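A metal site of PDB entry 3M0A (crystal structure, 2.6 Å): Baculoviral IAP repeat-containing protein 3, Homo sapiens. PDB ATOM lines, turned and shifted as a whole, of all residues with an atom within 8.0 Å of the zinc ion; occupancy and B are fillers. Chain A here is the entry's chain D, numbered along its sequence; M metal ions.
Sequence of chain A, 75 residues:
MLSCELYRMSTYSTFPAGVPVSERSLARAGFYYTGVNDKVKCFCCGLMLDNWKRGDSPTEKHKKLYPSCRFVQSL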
ATOM      1  N   ALA A  29       9.257  13.639 -13.443  1.00  0.00           N
ATOM      2  CA  ALA A  29       8.187  14.628 -13.240  1.00  0.00           C
ATOM      3  C   ALA A  29       8.638  15.818 -12.414  1.00  0.00           C
ATOM      4  O   ALA A  29       7.854  16.758 -12.162  1.00  0.00           O
ATOM      5  CB  ALA A  29       6.924  14.026 -12.613  1.00  0.00           C
ATOM      6  N   GLY A  30       9.899  15.775 -11.969  1.00  0.00           N
ATOM      7  CA  GLY A  30      10.519  16.868 -11.200  1.00  0.00           C
ATOM      8  C   GLY A  30      10.628  16.679  -9.712  1.00  0.00           C
ATOM      9  O   GLY A  30      10.920  17.669  -8.992  1.00  0.00           O
ATOM     10  N   PHE A  31      10.434  15.455  -9.213  1.00  0.00           N
ATOM     11  CA  PHE A  31      10.346  15.220  -7.765  1.00  0.00           C
ATOM     12  C   PHE A  31      11.561  14.463  -7.339  1.00  0.00           C
ATOM     13  O   PHE A  31      11.908  13.467  -8.057  1.00  0.00           O
ATOM     14  CB  PHE A  31       9.232  14.222  -7.457  1.00  0.00           C
ATOM     15  CG  PHE A  31       7.890  14.744  -7.717  1.00  0.00           C
ATOM     16  CD1 PHE A  31       7.356  15.746  -6.866  1.00  0.00           C
ATOM     17  CD2 PHE A  31       7.163  14.294  -8.817  1.00  0.00           C
ATOM     18  CE1 PHE A  31       6.054  16.300  -7.092  1.00  0.00           C
ATOM     19  CE2 PHE A  31       5.893  14.809  -9.059  1.00  0.00           C
ATOM     20  CZ  PHE A  31       5.329  15.838  -8.161  1.00  0.00           C
ATOM     21  N   LYS A  41       9.407  15.102  -3.348  1.00  0.00           N
ATOM     22  CA  LYS A  41       9.177  16.542  -3.366  1.00  0.00           C
ATOM     23  C   LYS A  41       9.709  17.260  -4.640  1.00  0.00           C
ATOM     24  O   LYS A  41      10.831  16.999  -5.089  1.00  0.00           O
ATOM     25  CB  LYS A  41       9.784  17.094  -2.076  1.00  0.00           C
ATOM     26  CG  LYS A  41       9.588  18.606  -1.826  1.00  0.00           C
ATOM     27  CD  LYS A  41      10.423  19.049  -0.636  1.00  0.00           C
ATOM     28  CE  LYS A  41      10.174  20.487  -0.331  1.00  0.00           C
ATOM     29  NZ  LYS A  41      10.843  20.775   0.965  1.00  0.00           N
ATOM     30  N   CYS A  42       8.904  18.148  -5.227  1.00  0.00           N
ATOM     31  CA  CYS A  42       9.296  18.725  -6.498  1.00  0.00           C
ATOM     32  C   CYS A  42      10.317  19.779  -6.148  1.00  0.00           C
ATOM     33  O   CYS A  42      10.037  20.689  -5.350  1.00  0.00           O
ATOM     34  CB  CYS A  42       8.106  19.351  -7.230  1.00  0.00           C
ATOM     35  SG  CYS A  42       8.596  20.579  -8.612  1.00  0.00           S
ATOM     36  N   PHE A  43      11.508  19.658  -6.745  1.00  0.00           N
ATOM     37  CA  PHE A  43      12.569  20.679  -6.476  1.00  0.00           C
ATOM     38  C   PHE A  43      12.133  22.127  -6.815  1.00  0.00           C
ATOM     39  O   PHE A  43      12.738  23.089  -6.378  1.00  0.00           O
ATOM     40  CB  PHE A  43      13.843  20.377  -7.274  1.00  0.00           C
ATOM     41  CG  PHE A  43      13.747  20.781  -8.691  1.00  0.00           C
ATOM     42  CD1 PHE A  43      14.519  21.836  -9.184  1.00  0.00           C
ATOM     43  CD2 PHE A  43      12.842  20.131  -9.555  1.00  0.00           C
ATOM     44  CE1 PHE A  43      14.420  22.289 -10.578  1.00  0.00           C
ATOM     45  CE2 PHE A  43      12.721  20.556 -10.949  1.00  0.00           C
ATOM     46  CZ  PHE A  43      13.527  21.644 -11.467  1.00  0.00           C
ATOM     47  N   CYS A  44      11.122  22.244  -7.651  1.00  0.00           N
ATOM     48  CA  CYS A  44      10.706  23.542  -8.095  1.00  0.00           C
ATOM     49  C   CYS A  44       9.661  24.172  -7.175  1.00  0.00           C
ATOM     50  O   CYS A  44       9.811  25.296  -6.656  1.00  0.00           O
ATOM     51  CB  CYS A  44      10.139  23.424  -9.493  1.00  0.00           C
ATOM     52  SG  CYS A  44       9.980  25.066 -10.211  1.00  0.00           S
ATOM     53  N   CYS A  45       8.560  23.478  -6.996  1.00  0.00           N
ATOM     54  CA  CYS A  45       7.453  24.157  -6.375  1.00  0.00           C
ATOM     55  C   CYS A  45       7.314  23.814  -4.907  1.00  0.00           C
ATOM     56  O   CYS A  45       6.608  24.509  -4.186  1.00  0.00           O
ATOM     57  CB  CYS A  45       6.193  23.861  -7.144  1.00  0.00           C
ATOM     58  SG  CYS A  45       5.852  22.149  -7.123  1.00  0.00           S
ATOM     59  N   GLY A  46       7.985  22.736  -4.475  1.00  0.00           N
ATOM     60  CA  GLY A  46       7.921  22.259  -3.068  1.00  0.00           C
ATOM     61  C   GLY A  46       6.773  21.292  -2.756  1.00  0.00           C
ATOM     62  O   GLY A  46       6.502  20.936  -1.561  1.00  0.00           O
ATOM     63  N   LEU A  47       6.111  20.846  -3.839  1.00  0.00           N
ATOM     64  CA  LEU A  47       4.923  19.992  -3.771  1.00  0.00           C
ATOM     65  C   LEU A  47       5.296  18.629  -3.233  1.00  0.00           C
ATOM     66  O   LEU A  47       6.196  17.965  -3.783  1.00  0.00           O
ATOM     67  CB  LEU A  47       4.224  19.875  -5.145  1.00  0.00           C
ATOM     68  CG  LEU A  47       3.161  18.789  -5.410  1.00  0.00           C
ATOM     69  CD1 LEU A  47       1.898  18.983  -4.611  1.00  0.00           C
ATOM     70  CD2 LEU A  47       2.789  18.708  -6.867  1.00  0.00           C
ATOM     71  N   HIS A  62       1.066  15.909 -10.730  1.00  0.00           N
ATOM     72  CA  HIS A  62       1.818  17.195 -10.601  1.00  0.00           C
ATOM     73  C   HIS A  62       0.908  18.281 -11.232  1.00  0.00           C
ATOM     74  O   HIS A  62       0.387  19.127 -10.491  1.00  0.00           O
ATOM     75  CB  HIS A  62       3.254  17.107 -11.248  1.00  0.00           C
ATOM     76  CG  HIS A  62       4.300  18.105 -10.754  1.00  0.00           C
ATOM     77  ND1 HIS A  62       5.609  18.061 -11.184  1.00  0.00           N
ATOM     78  CD2 HIS A  62       4.224  19.156  -9.888  1.00  0.00           C
ATOM     79  CE1 HIS A  62       6.292  19.044 -10.612  1.00  0.00           C
ATOM     80  NE2 HIS A  62       5.479  19.711  -9.812  1.00  0.00           N
ATOM     81  N   LYS A  63       0.663  18.238 -12.566  1.00  0.00           N
ATOM     82  CA  LYS A  63      -0.242  19.232 -13.268  1.00  0.00           C
ATOM     83  C   LYS A  63      -1.571  19.536 -12.466  1.00  0.00           C
ATOM     84  O   LYS A  63      -1.836  20.693 -12.140  1.00  0.00           O
ATOM     85  CB  LYS A  63      -0.471  18.870 -14.772  1.00  0.00           C
ATOM     86  N   TYR A  66      -0.837  21.661  -8.747  1.00  0.00           N
ATOM     87  CA  TYR A  66      -0.020  22.882  -8.663  1.00  0.00           C
ATOM     88  C   TYR A  66       0.491  23.289 -10.052  1.00  0.00           C
ATOM     89  O   TYR A  66       1.654  23.052 -10.373  1.00  0.00           O
ATOM     90  CB  TYR A  66       1.171  22.626  -7.751  1.00  0.00           C
ATOM     91  CG  TYR A  66       1.804  23.853  -7.117  1.00  0.00           C
ATOM     92  CD1 TYR A  66       1.852  23.994  -5.725  1.00  0.00           C
ATOM     93  CD2 TYR A  66       2.370  24.869  -7.906  1.00  0.00           C
ATOM     94  CE1 TYR A  66       2.435  25.102  -5.129  1.00  0.00           C
ATOM     95  CE2 TYR A  66       2.953  26.001  -7.314  1.00  0.00           C
ATOM     96  CZ  TYR A  66       2.985  26.109  -5.927  1.00  0.00           C
ATOM     97  OH  TYR A  66       3.587  27.202  -5.349  1.00  0.00           O
ATOM     98  N   PRO A  67      -0.383  23.878 -10.886  1.00  0.00           N
ATOM     99  CA  PRO A  67      -0.032  24.058 -12.306  1.00  0.00           C
ATOM    100  C   PRO A  67       0.817  25.317 -12.580  1.00  0.00           C
ATOM    101  O   PRO A  67       1.338  25.484 -13.699  1.00  0.00           O
ATOM    102  CB  PRO A  67      -1.394  24.131 -13.008  1.00  0.00           C
ATOM    103  CG  PRO A  67      -2.446  24.153 -11.863  1.00  0.00           C
ATOM    104  CD  PRO A  67      -1.729  24.386 -10.570  1.00  0.00           C
ATOM    105  N   SER A  68       0.970  26.159 -11.540  1.00  0.00           N
ATOM    106  CA  SER A  68       1.743  27.428 -11.563  1.00  0.00           C
ATOM    107  C   SER A  68       3.249  27.218 -11.565  1.00  0.00           C
ATOM    108  O   SER A  68       4.023  28.184 -11.548  1.00  0.00           O
ATOM    109  CB  SER A  68       1.375  28.307 -10.337  1.00  0.00           C
ATOM    110  OG  SER A  68       0.967  27.515  -9.224  1.00  0.00           O
ATOM    111  N   CYS A  69       3.624  25.943 -11.494  1.00  0.00           N
ATOM    112  CA  CYS A  69       5.009  25.545 -11.278  1.00  0.00           C
ATOM    113  C   CYS A  69       5.804  25.810 -12.541  1.00  0.00           C
ATOM    114  O   CYS A  69       5.517  25.257 -13.600  1.00  0.00           O
ATOM    115  CB  CYS A  69       5.082  24.073 -10.872  1.00  0.00           C
ATOM    116  SG  CYS A  69       6.767  23.447 -10.626  1.00  0.00           S
ATOM    117  N   ARG A  70       6.797  26.678 -12.422  1.00  0.00           N
ATOM    118  CA  ARG A  70       7.656  26.973 -13.538  1.00  0.00           C
ATOM    119  C   ARG A  70       8.115  25.713 -14.179  1.00  0.00           C
ATOM    120  O   ARG A  70       8.273  25.650 -15.379  1.00  0.00           O
ATOM    121  CB  ARG A  70       8.868  27.759 -13.090  1.00  0.00           C
ATOM    122  N   PHE A  71       8.367  24.692 -13.381  1.00  0.00           N
ATOM    123  CA  PHE A  71       8.784  23.384 -13.924  1.00  0.00           C
ATOM    124  C   PHE A  71       7.683  22.621 -14.649  1.00  0.00           C
ATOM    125  O   PHE A  71       7.884  22.160 -15.766  1.00  0.00           O
ATOM    126  CB  PHE A  71       9.382  22.451 -12.873  1.00  0.00           C
ATOM    127  CG  PHE A  71       9.981  21.198 -13.470  1.00  0.00           C
ATOM    128  CD1 PHE A  71      11.094  21.259 -14.293  1.00  0.00           C
ATOM    129  CD2 PHE A  71       9.404  19.961 -13.260  1.00  0.00           C
ATOM    130  CE1 PHE A  71      11.647  20.094 -14.880  1.00  0.00           C
ATOM    131  CE2 PHE A  71       9.942  18.788 -13.855  1.00  0.00           C
ATOM    132  CZ  PHE A  71      11.063  18.863 -14.664  1.00  0.00           C
ATOM    133  N   VAL A  72       6.538  22.466 -13.986  1.00  0.00           N
ATOM    134  CA  VAL A  72       5.459  21.656 -14.525  1.00  0.00           C
ATOM    135  C   VAL A  72       5.008  22.152 -15.897  1.00  0.00           C
ATOM    136  O   VAL A  72       4.523  21.356 -16.706  1.00  0.00           O
ATOM    137  CB  VAL A  72       4.221  21.584 -13.589  1.00  0.00           C
ATOM    138  CG1 VAL A  72       3.546  22.929 -13.464  1.00  0.00           C
ATOM    139  CG2 VAL A  72       3.234  20.575 -14.129  1.00  0.00           C
ATOM    140  N   GLN A  73       5.203  23.470 -16.116  1.00  0.00           N
ATOM    141  CA  GLN A  73       4.837  24.193 -17.350  1.00  0.00           C
ATOM    142  C   GLN A  73       5.242  23.374 -18.587  1.00  0.00           C
ATOM    143  O   GLN A  73       4.552  23.466 -19.632  1.00  0.00           O
ATOM    144  CB  GLN A  73       5.441  25.609 -17.410  1.00  0.00           C
ATOM    145  CG  GLN A  73       4.422  26.777 -17.563  1.00  0.00           C
ATOM    146  CD  GLN A  73       3.751  27.208 -16.215  1.00  0.00           C
ATOM    147  OE1 GLN A  73       3.994  28.319 -15.686  1.00  0.00           O
ATOM    148  NE2 GLN A  73       2.912  26.323 -15.668  1.00  0.00           N
HETATM  149 ZN    ZN M   1       6.687  21.506  -9.244  1.00  0.00          ZN
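The side-chain sulfur (SG) of Cys 69 sits close to the backbone NH (N) of Val 72 (3.5 Å).
NE2 of Gln 73 sits at hydrogen-bond distance from O of Cys 69 (3.5 Å).
The side-chain sulfur (SG) of Cys 45 lies close to the backbone NH (N) of Leu 47.
The side-chain sulfur of Cys 42 lies close to the backbone NH of Cys 44.
SG of Cys 69 lies close to N of Phe 71.
ND1 of His 62 lies within hydrogen-bond range of O of Ala 29 (2.8 Å).
N of Cys 42 lies within hydrogen-bond range of O of Leu 47 (3.1 Å).
The side-chain sulfur (SG) of Cys 44 is in hydrogen-bond range of the backbone NH (N) of Phe 71, 3.6 Å away.
Merely in contact with the zinc ion: Cys 44.
The nearest printed residue that does not touch the zinc ion is Phe 71 (4.6 Å).
The zinc ion is bound by the side-chain sulfur of Cys 42 (2.2 Å), a ring nitrogen (NE2) of His 62 (2.2 Å), the side-chain sulfur of Cys 45 (2.4 Å) and the side-chain sulfur of Cys 69 (2.4 Å).
The zinc ion has four donor atoms within binding distance.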
